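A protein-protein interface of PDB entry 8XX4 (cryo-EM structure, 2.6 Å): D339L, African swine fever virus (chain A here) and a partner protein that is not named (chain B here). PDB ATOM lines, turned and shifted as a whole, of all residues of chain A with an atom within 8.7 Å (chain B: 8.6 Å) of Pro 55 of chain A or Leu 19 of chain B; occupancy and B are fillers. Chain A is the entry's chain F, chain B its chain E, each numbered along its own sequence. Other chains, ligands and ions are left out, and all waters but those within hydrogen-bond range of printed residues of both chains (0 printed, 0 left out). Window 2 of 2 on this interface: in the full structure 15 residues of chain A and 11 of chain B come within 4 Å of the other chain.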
ATOM      1  N   THR A   9       8.834   6.991 -22.486  1.00  0.00           N
ATOM      2  CA  THR A   9       8.103   8.186 -22.097  1.00  0.00           C
ATOM      3  C   THR A   9       8.511   9.305 -23.043  1.00  0.00           C
ATOM      4  O   THR A   9       9.699   9.608 -23.175  1.00  0.00           O
ATOM      5  CB  THR A   9       8.369   8.559 -20.636  1.00  0.00           C
ATOM      6  OG1 THR A   9       7.907   9.889 -20.378  1.00  0.00           O
ATOM      7  CG2 THR A   9       9.839   8.455 -20.292  1.00  0.00           C
ATOM      8  N   LEU A  10       7.534   9.888 -23.723  1.00  0.00           N
ATOM      9  CA  LEU A  10       7.800  10.964 -24.657  1.00  0.00           C
ATOM     10  C   LEU A  10       7.890  12.287 -23.908  1.00  0.00           C
ATOM     11  O   LEU A  10       7.667  12.364 -22.702  1.00  0.00           O
ATOM     12  CB  LEU A  10       6.718  11.021 -25.731  1.00  0.00           C
ATOM     13  CG  LEU A  10       6.750   9.941 -26.807  1.00  0.00           C
ATOM     14  CD1 LEU A  10       6.046  10.436 -28.044  1.00  0.00           C
ATOM     15  CD2 LEU A  10       8.167   9.530 -27.128  1.00  0.00           C
ATOM     16  N   ILE A  12       6.315  16.194 -24.510  1.00  0.00           N
ATOM     17  CA  ILE A  12       5.328  16.910 -25.301  1.00  0.00           C
ATOM     18  C   ILE A  12       5.502  18.393 -25.024  1.00  0.00           C
ATOM     19  O   ILE A  12       5.109  18.886 -23.961  1.00  0.00           O
ATOM     20  CB  ILE A  12       3.905  16.445 -24.988  1.00  0.00           C
ATOM     21  CG1 ILE A  12       3.757  14.969 -25.345  1.00  0.00           C
ATOM     22  CG2 ILE A  12       2.922  17.264 -25.755  1.00  0.00           C
ATOM     23  CD1 ILE A  12       2.761  14.246 -24.506  1.00  0.00           C
ATOM     24  N   PHE A  18      -0.937  19.017 -28.980  1.00  0.00           N
ATOM     25  CA  PHE A  18      -0.718  17.579 -29.072  1.00  0.00           C
ATOM     26  C   PHE A  18      -2.000  16.805 -28.808  1.00  0.00           C
ATOM     27  O   PHE A  18      -2.277  15.802 -29.472  1.00  0.00           O
ATOM     28  CB  PHE A  18       0.370  17.176 -28.081  1.00  0.00           C
ATOM     29  CG  PHE A  18       0.768  15.733 -28.148  1.00  0.00           C
ATOM     30  CD1 PHE A  18       1.787  15.321 -28.982  1.00  0.00           C
ATOM     31  CD2 PHE A  18       0.150  14.795 -27.345  1.00  0.00           C
ATOM     32  CE1 PHE A  18       2.163  14.000 -29.030  1.00  0.00           C
ATOM     33  CE2 PHE A  18       0.521  13.475 -27.393  1.00  0.00           C
ATOM     34  CZ  PHE A  18       1.528  13.077 -28.236  1.00  0.00           C
ATOM     35  N   CYS A  19      -2.797  17.258 -27.845  1.00  0.00           N
ATOM     36  CA  CYS A  19      -3.995  16.540 -27.439  1.00  0.00           C
ATOM     37  C   CYS A  19      -5.158  16.718 -28.402  1.00  0.00           C
ATOM     38  O   CYS A  19      -6.192  16.067 -28.220  1.00  0.00           O
ATOM     39  CB  CYS A  19      -4.409  16.981 -26.036  1.00  0.00           C
ATOM     40  SG  CYS A  19      -3.420  16.231 -24.737  1.00  0.00           S
ATOM     41  N   VAL A  22      -4.275  12.895 -30.406  1.00  0.00           N
ATOM     42  CA  VAL A  22      -3.238  12.218 -29.634  1.00  0.00           C
ATOM     43  C   VAL A  22      -2.647  11.051 -30.413  1.00  0.00           C
ATOM     44  O   VAL A  22      -1.432  10.845 -30.404  1.00  0.00           O
ATOM     45  CB  VAL A  22      -3.785  11.771 -28.268  1.00  0.00           C
ATOM     46  CG1 VAL A  22      -2.937  10.652 -27.700  1.00  0.00           C
ATOM     47  CG2 VAL A  22      -3.791  12.937 -27.317  1.00  0.00           C
ATOM     48  N   GLN A  52      -0.424   0.766 -25.789  1.00  0.00           N
ATOM     49  CA  GLN A  52      -0.799   1.269 -24.481  1.00  0.00           C
ATOM     50  C   GLN A  52      -0.112   2.609 -24.304  1.00  0.00           C
ATOM     51  O   GLN A  52       1.028   2.781 -24.736  1.00  0.00           O
ATOM     52  CB  GLN A  52      -0.382   0.303 -23.371  1.00  0.00           C
ATOM     53  CG  GLN A  52      -1.505  -0.169 -22.484  1.00  0.00           C
ATOM     54  CD  GLN A  52      -1.018  -1.120 -21.416  1.00  0.00           C
ATOM     55  OE1 GLN A  52      -0.084  -1.887 -21.636  1.00  0.00           O
ATOM     56  NE2 GLN A  52      -1.647  -1.076 -20.250  1.00  0.00           N
ATOM     57  N   ARG A  53      -0.805   3.554 -23.683  1.00  0.00           N
ATOM     58  CA  ARG A  53      -0.223   4.860 -23.430  1.00  0.00           C
ATOM     59  C   ARG A  53      -0.742   5.364 -22.092  1.00  0.00           C
ATOM     60  O   ARG A  53      -1.456   4.662 -21.371  1.00  0.00           O
ATOM     61  CB  ARG A  53      -0.531   5.832 -24.573  1.00  0.00           C
ATOM     62  CG  ARG A  53      -1.979   5.856 -24.979  1.00  0.00           C
ATOM     63  CD  ARG A  53      -2.297   7.096 -25.773  1.00  0.00           C
ATOM     64  NE  ARG A  53      -2.698   8.190 -24.902  1.00  0.00           N
ATOM     65  CZ  ARG A  53      -3.887   8.774 -24.937  1.00  0.00           C
ATOM     66  NH1 ARG A  53      -4.817   8.396 -25.795  1.00  0.00           N
ATOM     67  NH2 ARG A  53      -4.147   9.760 -24.087  1.00  0.00           N
ATOM     68  N   SER A  54      -0.381   6.590 -21.768  1.00  0.00           N
ATOM     69  CA  SER A  54      -0.733   7.244 -20.521  1.00  0.00           C
ATOM     70  C   SER A  54      -1.438   8.549 -20.833  1.00  0.00           C
ATOM     71  O   SER A  54      -1.362   9.053 -21.958  1.00  0.00           O
ATOM     72  CB  SER A  54       0.515   7.524 -19.676  1.00  0.00           C
ATOM     73  OG  SER A  54       0.976   8.846 -19.883  1.00  0.00           O
ATOM     74  N   PRO A  55      -2.157   9.112 -19.867  1.00  0.00           N
ATOM     75  CA  PRO A  55      -2.601  10.497 -20.010  1.00  0.00           C
ATOM     76  C   PRO A  55      -1.399  11.422 -20.121  1.00  0.00           C
ATOM     77  O   PRO A  55      -0.306  11.115 -19.647  1.00  0.00           O
ATOM     78  CB  PRO A  55      -3.391  10.752 -18.724  1.00  0.00           C
ATOM     79  CG  PRO A  55      -3.804   9.411 -18.268  1.00  0.00           C
ATOM     80  CD  PRO A  55      -2.721   8.473 -18.669  1.00  0.00           C
ATOM     81  N   CYS A  56      -1.601  12.553 -20.787  1.00  0.00           N
ATOM     82  CA  CYS A  56      -0.517  13.511 -20.934  1.00  0.00           C
ATOM     83  C   CYS A  56      -0.298  14.249 -19.622  1.00  0.00           C
ATOM     84  O   CYS A  56      -0.857  15.328 -19.411  1.00  0.00           O
ATOM     85  CB  CYS A  56      -0.811  14.495 -22.067  1.00  0.00           C
ATOM     86  SG  CYS A  56       0.423  15.796 -22.271  1.00  0.00           S
ATOM     87  N   PHE A  57       0.498  13.666 -18.732  1.00  0.00           N
ATOM     88  CA  PHE A  57       0.790  14.306 -17.458  1.00  0.00           C
ATOM     89  C   PHE A  57       1.603  15.570 -17.676  1.00  0.00           C
ATOM     90  O   PHE A  57       2.537  15.590 -18.473  1.00  0.00           O
ATOM     91  CB  PHE A  57       1.567  13.363 -16.548  1.00  0.00           C
ATOM     92  CG  PHE A  57       0.967  12.003 -16.418  1.00  0.00           C
ATOM     93  CD1 PHE A  57      -0.171  11.806 -15.669  1.00  0.00           C
ATOM     94  CD2 PHE A  57       1.556  10.916 -17.024  1.00  0.00           C
ATOM     95  CE1 PHE A  57      -0.716  10.556 -15.542  1.00  0.00           C
ATOM     96  CE2 PHE A  57       1.013   9.664 -16.895  1.00  0.00           C
ATOM     97  CZ  PHE A  57      -0.126   9.486 -16.154  1.00  0.00           C
ATOM     98  N   ILE A  58       1.257  16.619 -16.954  1.00  0.00           N
ATOM     99  CA  ILE A  58       2.028  17.854 -16.998  1.00  0.00           C
ATOM    100  C   ILE A  58       3.277  17.685 -16.151  1.00  0.00           C
ATOM    101  O   ILE A  58       3.223  17.144 -15.042  1.00  0.00           O
ATOM    102  CB  ILE A  58       1.176  19.040 -16.518  1.00  0.00           C
ATOM    103  CG1 ILE A  58       0.002  19.261 -17.467  1.00  0.00           C
ATOM    104  CG2 ILE A  58       2.012  20.296 -16.430  1.00  0.00           C
ATOM    105  CD1 ILE A  58       0.382  19.169 -18.909  1.00  0.00           C
ATOM    106  N   GLY A  67       4.176  18.503 -21.095  1.00  0.00           N
ATOM    107  CA  GLY A  67       3.705  17.202 -20.669  1.00  0.00           C
ATOM    108  C   GLY A  67       4.625  16.114 -21.163  1.00  0.00           C
ATOM    109  O   GLY A  67       5.468  16.387 -22.018  1.00  0.00           O
ATOM    110  N   TYR A  68       4.520  14.889 -20.646  1.00  0.00           N
ATOM    111  CA  TYR A  68       5.407  13.836 -21.127  1.00  0.00           C
ATOM    112  C   TYR A  68       4.675  12.668 -21.775  1.00  0.00           C
ATOM    113  O   TYR A  68       4.968  12.357 -22.933  1.00  0.00           O
ATOM    114  CB  TYR A  68       6.346  13.339 -20.018  1.00  0.00           C
ATOM    115  CG  TYR A  68       5.780  13.171 -18.632  1.00  0.00           C
ATOM    116  CD1 TYR A  68       5.546  14.267 -17.815  1.00  0.00           C
ATOM    117  CD2 TYR A  68       5.551  11.911 -18.113  1.00  0.00           C
ATOM    118  CE1 TYR A  68       5.062  14.109 -16.544  1.00  0.00           C
ATOM    119  CE2 TYR A  68       5.070  11.748 -16.845  1.00  0.00           C
ATOM    120  CZ  TYR A  68       4.829  12.850 -16.064  1.00  0.00           C
ATOM    121  OH  TYR A  68       4.345  12.687 -14.792  1.00  0.00           O
ATOM    122  N   MET A  69       3.748  12.008 -21.081  1.00  0.00           N
ATOM    123  CA  MET A  69       3.086  10.801 -21.584  1.00  0.00           C
ATOM    124  C   MET A  69       4.028   9.612 -21.739  1.00  0.00           C
ATOM    125  O   MET A  69       5.042   9.694 -22.434  1.00  0.00           O
ATOM    126  CB  MET A  69       2.392  11.058 -22.927  1.00  0.00           C
ATOM    127  CG  MET A  69       1.454   9.951 -23.362  1.00  0.00           C
ATOM    128  SD  MET A  69       0.628  10.308 -24.914  1.00  0.00           S
ATOM    129  CE  MET A  69      -0.524  11.570 -24.400  1.00  0.00           C
ATOM    130  N   HIS A  70       3.685   8.498 -21.098  1.00  0.00           N
ATOM    131  CA  HIS A  70       4.344   7.223 -21.333  1.00  0.00           C
ATOM    132  C   HIS A  70       3.592   6.462 -22.413  1.00  0.00           C
ATOM    133  O   HIS A  70       2.361   6.424 -22.412  1.00  0.00           O
ATOM    134  CB  HIS A  70       4.384   6.382 -20.059  1.00  0.00           C
ATOM    135  CG  HIS A  70       4.733   7.156 -18.830  1.00  0.00           C
ATOM    136  ND1 HIS A  70       6.011   7.592 -18.566  1.00  0.00           N
ATOM    137  CD2 HIS A  70       3.973   7.562 -17.788  1.00  0.00           C
ATOM    138  CE1 HIS A  70       6.023   8.237 -17.415  1.00  0.00           C
ATOM    139  NE2 HIS A  70       4.799   8.233 -16.923  1.00  0.00           N
ATOM    140  N   VAL A  71       4.332   5.860 -23.338  1.00  0.00           N
ATOM    141  CA  VAL A  71       3.732   5.102 -24.427  1.00  0.00           C
ATOM    142  C   VAL A  71       4.474   3.785 -24.585  1.00  0.00           C
ATOM    143  O   VAL A  71       5.692   3.772 -24.792  1.00  0.00           O
ATOM    144  CB  VAL A  71       3.738   5.894 -25.749  1.00  0.00           C
ATOM    145  CG1 VAL A  71       5.015   6.685 -25.894  1.00  0.00           C
ATOM    146  CG2 VAL A  71       3.555   4.957 -26.927  1.00  0.00           C
ATOM    147  N   SER B  16       6.355  -1.728 -14.410  1.00  0.00           N
ATOM    148  CA  SER B  16       5.491  -0.700 -14.966  1.00  0.00           C
ATOM    149  C   SER B  16       4.076  -0.881 -14.436  1.00  0.00           C
ATOM    150  O   SER B  16       3.612  -2.003 -14.224  1.00  0.00           O
ATOM    151  CB  SER B  16       5.504  -0.765 -16.488  1.00  0.00           C
ATOM    152  OG  SER B  16       4.744   0.289 -17.035  1.00  0.00           O
ATOM    153  N   GLN B  17       3.396   0.230 -14.203  1.00  0.00           N
ATOM    154  CA  GLN B  17       2.096   0.209 -13.558  1.00  0.00           C
ATOM    155  C   GLN B  17       0.979   0.448 -14.564  1.00  0.00           C
ATOM    156  O   GLN B  17       1.185   1.005 -15.641  1.00  0.00           O
ATOM    157  CB  GLN B  17       2.039   1.253 -12.443  1.00  0.00           C
ATOM    158  CG  GLN B  17       3.265   1.246 -11.562  1.00  0.00           C
ATOM    159  CD  GLN B  17       3.189   2.249 -10.437  1.00  0.00           C
ATOM    160  OE1 GLN B  17       2.819   3.402 -10.639  1.00  0.00           O
ATOM    161  NE2 GLN B  17       3.549   1.815  -9.240  1.00  0.00           N
ATOM    162  N   THR B  18      -0.213  -0.007 -14.202  1.00  0.00           N
ATOM    163  CA  THR B  18      -1.419   0.245 -14.971  1.00  0.00           C
ATOM    164  C   THR B  18      -2.285   1.230 -14.206  1.00  0.00           C
ATOM    165  O   THR B  18      -2.506   1.062 -13.004  1.00  0.00           O
ATOM    166  CB  THR B  18      -2.197  -1.045 -15.244  1.00  0.00           C
ATOM    167  OG1 THR B  18      -2.099  -1.917 -14.112  1.00  0.00           O
ATOM    168  CG2 THR B  18      -1.650  -1.746 -16.475  1.00  0.00           C
ATOM    169  N   LEU B  19      -2.757   2.258 -14.899  1.00  0.00           N
ATOM    170  CA  LEU B  19      -3.582   3.283 -14.280  1.00  0.00           C
ATOM    171  C   LEU B  19      -4.965   2.718 -13.998  1.00  0.00           C
ATOM    172  O   LEU B  19      -5.686   2.337 -14.924  1.00  0.00           O
ATOM    173  CB  LEU B  19      -3.673   4.502 -15.190  1.00  0.00           C
ATOM    174  CG  LEU B  19      -3.985   5.851 -14.559  1.00  0.00           C
ATOM    175  CD1 LEU B  19      -2.865   6.280 -13.636  1.00  0.00           C
ATOM    176  CD2 LEU B  19      -4.196   6.866 -15.652  1.00  0.00           C
ATOM    177  N   VAL B  20      -5.333   2.658 -12.725  1.00  0.00           N
ATOM    178  CA  VAL B  20      -6.653   2.212 -12.304  1.00  0.00           C
ATOM    179  C   VAL B  20      -7.440   3.465 -11.948  1.00  0.00           C
ATOM    180  O   VAL B  20      -7.222   4.072 -10.898  1.00  0.00           O
ATOM    181  CB  VAL B  20      -6.580   1.233 -11.131  1.00  0.00           C
ATOM    182  CG1 VAL B  20      -7.971   0.858 -10.683  1.00  0.00           C
ATOM    183  CG2 VAL B  20      -5.803   0.002 -11.527  1.00  0.00           C
ATOM    184  N   ILE B  21      -8.352   3.860 -12.823  1.00  0.00           N
ATOM    185  CA  ILE B  21      -9.169   5.043 -12.599  1.00  0.00           C
ATOM    186  C   ILE B  21     -10.395   4.629 -11.801  1.00  0.00           C
ATOM    187  O   ILE B  21     -11.183   3.789 -12.245  1.00  0.00           O
ATOM    188  CB  ILE B  21      -9.563   5.711 -13.924  1.00  0.00           C
ATOM    189  CG1 ILE B  21      -8.333   6.325 -14.589  1.00  0.00           C
ATOM    190  CG2 ILE B  21     -10.593   6.786 -13.682  1.00  0.00           C
ATOM    191  CD1 ILE B  21      -8.428   6.419 -16.086  1.00  0.00           C
ATOM    192  N   ILE B  22     -10.543   5.204 -10.618  1.00  0.00           N
ATOM    193  CA  ILE B  22     -11.709   4.923  -9.775  1.00  0.00           C
ATOM    194  C   ILE B  22     -12.961   5.428 -10.477  1.00  0.00           C
ATOM    195  O   ILE B  22     -12.961   6.561 -10.988  1.00  0.00           O
ATOM    196  CB  ILE B  22     -11.537   5.581  -8.407  1.00  0.00           C
ATOM    197  CG1 ILE B  22     -10.541   4.790  -7.564  1.00  0.00           C
ATOM    198  CG2 ILE B  22     -12.859   5.683  -7.686  1.00  0.00           C
ATOM    199  CD1 ILE B  22     -10.268   5.402  -6.221  1.00  0.00           C
ATOM    200  N   LEU B  80      -7.352  18.401 -16.489  1.00  0.00           N
ATOM    201  CA  LEU B  80      -7.991  17.508 -15.538  1.00  0.00           C
ATOM    202  C   LEU B  80      -7.092  17.361 -14.319  1.00  0.00           C
ATOM    203  O   LEU B  80      -5.872  17.494 -14.404  1.00  0.00           O
ATOM    204  CB  LEU B  80      -8.268  16.126 -16.140  1.00  0.00           C
ATOM    205  CG  LEU B  80      -9.349  15.966 -17.204  1.00  0.00           C
ATOM    206  CD1 LEU B  80      -9.314  14.561 -17.745  1.00  0.00           C
ATOM    207  CD2 LEU B  80     -10.716  16.278 -16.645  1.00  0.00           C
ATOM    208  N   MET B  82      -5.869  14.781 -11.431  1.00  0.00           N
ATOM    209  CA  MET B  82      -5.771  13.367 -11.104  1.00  0.00           C
ATOM    210  C   MET B  82      -5.206  13.228  -9.698  1.00  0.00           C
ATOM    211  O   MET B  82      -4.100  13.699  -9.420  1.00  0.00           O
ATOM    212  CB  MET B  82      -4.908  12.619 -12.117  1.00  0.00           C
ATOM    213  CG  MET B  82      -4.470  11.255 -11.642  1.00  0.00           C
ATOM    214  SD  MET B  82      -2.977  10.665 -12.439  1.00  0.00           S
ATOM    215  CE  MET B  82      -3.686   9.968 -13.919  1.00  0.00           C
ATOM    216  N   ARG B  83      -5.964  12.587  -8.822  1.00  0.00           N
ATOM    217  CA  ARG B  83      -5.598  12.415  -7.424  1.00  0.00           C
ATOM    218  C   ARG B  83      -5.202  10.963  -7.213  1.00  0.00           C
ATOM    219  O   ARG B  83      -6.058  10.077  -7.214  1.00  0.00           O
ATOM    220  CB  ARG B  83      -6.756  12.813  -6.516  1.00  0.00           C
ATOM    221  CG  ARG B  83      -7.248  14.222  -6.745  1.00  0.00           C
ATOM    222  CD  ARG B  83      -8.431  14.535  -5.866  1.00  0.00           C
ATOM    223  NE  ARG B  83      -8.617  15.966  -5.685  1.00  0.00           N
ATOM    224  CZ  ARG B  83      -9.784  16.539  -5.435  1.00  0.00           C
ATOM    225  NH1 ARG B  83     -10.896  15.833  -5.356  1.00  0.00           N
ATOM    226  NH2 ARG B  83      -9.836  17.855  -5.258  1.00  0.00           N
ATOM    227  N   CYS B  84      -3.908  10.720  -7.034  1.00  0.00           N
ATOM    228  CA  CYS B  84      -3.398   9.368  -6.849  1.00  0.00           C
ATOM    229  C   CYS B  84      -3.692   8.927  -5.424  1.00  0.00           C
ATOM    230  O   CYS B  84      -3.120   9.459  -4.469  1.00  0.00           O
ATOM    231  CB  CYS B  84      -1.905   9.314  -7.147  1.00  0.00           C
ATOM    232  SG  CYS B  84      -1.169   7.673  -6.982  1.00  0.00           S
ATOM    233  N   LYS B  86      -3.809   5.414  -4.160  1.00  0.00           N
ATOM    234  CA  LYS B  86      -3.032   4.285  -3.682  1.00  0.00           C
ATOM    235  C   LYS B  86      -2.110   3.801  -4.786  1.00  0.00           C
ATOM    236  O   LYS B  86      -2.397   3.966  -5.972  1.00  0.00           O
ATOM    237  CB  LYS B  86      -3.948   3.146  -3.214  1.00  0.00           C
ATOM    238  CG  LYS B  86      -3.253   2.008  -2.497  1.00  0.00           C
ATOM    239  CD  LYS B  86      -2.321   2.517  -1.422  1.00  0.00           C
ATOM    240  CE  LYS B  86      -1.986   1.426  -0.425  1.00  0.00           C
ATOM    241  NZ  LYS B  86      -3.084   0.432  -0.312  1.00  0.00           N
ATOM    242  N   GLY B  91       1.248  -3.615  -9.045  1.00  0.00           N
ATOM    243  CA  GLY B  91       1.541  -2.835 -10.230  1.00  0.00           C
ATOM    244  C   GLY B  91       0.385  -1.968 -10.683  1.00  0.00           C
ATOM    245  O   GLY B  91       0.187  -1.764 -11.883  1.00  0.00           O
ATOM    246  N   GLN B  92      -0.386  -1.452  -9.734  1.00  0.00           N
ATOM    247  CA  GLN B  92      -1.594  -0.696 -10.028  1.00  0.00           C
ATOM    248  C   GLN B  92      -1.530   0.663  -9.354  1.00  0.00           C
ATOM    249  O   GLN B  92      -1.270   0.757  -8.152  1.00  0.00           O
ATOM    250  CB  GLN B  92      -2.833  -1.454  -9.555  1.00  0.00           C
ATOM    251  CG  GLN B  92      -3.072  -2.758 -10.288  1.00  0.00           C
ATOM    252  CD  GLN B  92      -4.541  -3.048 -10.494  1.00  0.00           C
ATOM    253  OE1 GLN B  92      -5.360  -2.813  -9.608  1.00  0.00           O
ATOM    254  NE2 GLN B  92      -4.884  -3.560 -11.669  1.00  0.00           N
ATOM    255  N   LYS B  93      -1.770   1.713 -10.127  1.00  0.00           N
ATOM    256  CA  LYS B  93      -1.815   3.078  -9.612  1.00  0.00           C
ATOM    257  C   LYS B  93      -3.276   3.502  -9.587  1.00  0.00           C
ATOM    258  O   LYS B  93      -3.867   3.786 -10.631  1.00  0.00           O
ATOM    259  CB  LYS B  93      -0.971   4.019 -10.460  1.00  0.00           C
ATOM    260  CG  LYS B  93      -0.838   5.406  -9.871  1.00  0.00           C
ATOM    261  CD  LYS B  93       0.486   6.036 -10.234  1.00  0.00           C
ATOM    262  CE  LYS B  93       0.283   7.318 -11.010  1.00  0.00           C
ATOM    263  NZ  LYS B  93       0.125   8.483 -10.103  1.00  0.00           N
ATOM    264  N   ILE B  94      -3.855   3.539  -8.394  1.00  0.00           N
ATOM    265  CA  ILE B  94      -5.269   3.856  -8.231  1.00  0.00           C
ATOM    266  C   ILE B  94      -5.417   5.366  -8.104  1.00  0.00           C
ATOM    267  O   ILE B  94      -4.867   5.978  -7.185  1.00  0.00           O
ATOM    268  CB  ILE B  94      -5.852   3.135  -7.011  1.00  0.00           C
ATOM    269  CG1 ILE B  94      -5.862   1.628  -7.242  1.00  0.00           C
ATOM    270  CG2 ILE B  94      -7.242   3.627  -6.723  1.00  0.00           C
ATOM    271  CD1 ILE B  94      -5.290   0.846  -6.100  1.00  0.00           C
ATOM    272  N   VAL B  95      -6.162   5.971  -9.029  1.00  0.00           N
ATOM    273  CA  VAL B  95      -6.312   7.416  -9.082  1.00  0.00           C
ATOM    274  C   VAL B  95      -7.787   7.774  -9.167  1.00  0.00           C
ATOM    275  O   VAL B  95      -8.636   6.952  -9.509  1.00  0.00           O
ATOM    276  CB  VAL B  95      -5.552   8.044 -10.270  1.00  0.00           C
ATOM    277  CG1 VAL B  95      -4.094   7.651 -10.240  1.00  0.00           C
ATOM    278  CG2 VAL B  95      -6.194   7.640 -11.578  1.00  0.00           C
ATOM    279  N   GLU B  96      -8.081   9.027  -8.835  1.00  0.00           N
ATOM    280  CA  GLU B  96      -9.391   9.625  -9.044  1.00  0.00           C
ATOM    281  C   GLU B  96      -9.216  10.812  -9.974  1.00  0.00           C
ATOM    282  O   GLU B  96      -8.523  11.772  -9.631  1.00  0.00           O
ATOM    283  CB  GLU B  96     -10.017  10.070  -7.724  1.00  0.00           C
ATOM    284  CG  GLU B  96     -10.452   8.932  -6.841  1.00  0.00           C
ATOM    285  CD  GLU B  96     -11.161   9.402  -5.597  1.00  0.00           C
ATOM    286  OE1 GLU B  96     -11.499  10.598  -5.530  1.00  0.00           O
ATOM    287  OE2 GLU B  96     -11.381   8.577  -4.688  1.00  0.00           O
ATOM    288  N   ILE B  97      -9.832  10.745 -11.146  1.00  0.00           N
ATOM    289  CA  ILE B  97      -9.745  11.820 -12.123  1.00  0.00           C
ATOM    290  C   ILE B  97     -10.929  12.751 -11.929  1.00  0.00           C
ATOM    291  O   ILE B  97     -12.086  12.325 -11.997  1.00  0.00           O
ATOM    292  CB  ILE B  97      -9.707  11.266 -13.554  1.00  0.00           C
ATOM    293  CG1 ILE B  97      -8.691  10.128 -13.653  1.00  0.00           C
ATOM    294  CG2 ILE B  97      -9.399  12.372 -14.537  1.00  0.00           C
ATOM    295  CD1 ILE B  97      -7.307  10.572 -14.014  1.00  0.00           C
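The backbone carbonyl oxygen (O) of Gly 91 of chain B lies within hydrogen-bond range of the backbone NH (N) of Thr 18 of chain B (2.9 Å).
The backbone carbonyl oxygen of Thr 18 of chain B sits at hydrogen-bond distance from the backbone NH of Lys 93 of chain B (3.0 Å).
The backbone carbonyl oxygen of Phe 57 of chain A sits at hydrogen-bond distance from the backbone NH of Tyr 68 of chain A (3.0 Å).
Among the printed residues, pairs that only touch across the chains: Gln 52 of chain A with Thr 18 of chain B (3.8 Å), Pro 55 of chain A with Leu 19 of chain B (3.7 Å) and Phe 57 of chain A with Met 82 of chain B (3.4 Å).
Of the printed residues of chain B, Gln 52 of chain A touches Thr 18.
No residue of chain B comes within 4 Å of Ser 54 of chain A.
Printed residues of chain B within 4 Å of Phe 57 of chain A: Met 82.
Of chain A, only Gln 52 (3.8 Å) comes within 4 Å of Thr 18 of chain B.
Leu 19 of chain B touches one residue of chain A.
Printed residues of chain A within 4 Å of Met 82 of chain B: Phe 57 (3.4 Å).
The nearest residue of chain A that does not touch Leu 19 of chain B is Phe 57 of chain A (4.9 Å).
Printed residues of chain B that touch a printed residue of chain A: Thr 18, Leu 19 and Met 82.
Hydrophobic or aromatic side chains of chain A within 4 Å of the printed part of chain B: Pro 55 and Phe 57.
Among the printed residues, no Asp or Glu carboxylate lies within 4 Å of a Lys or Arg side-chain nitrogen of the other chain.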
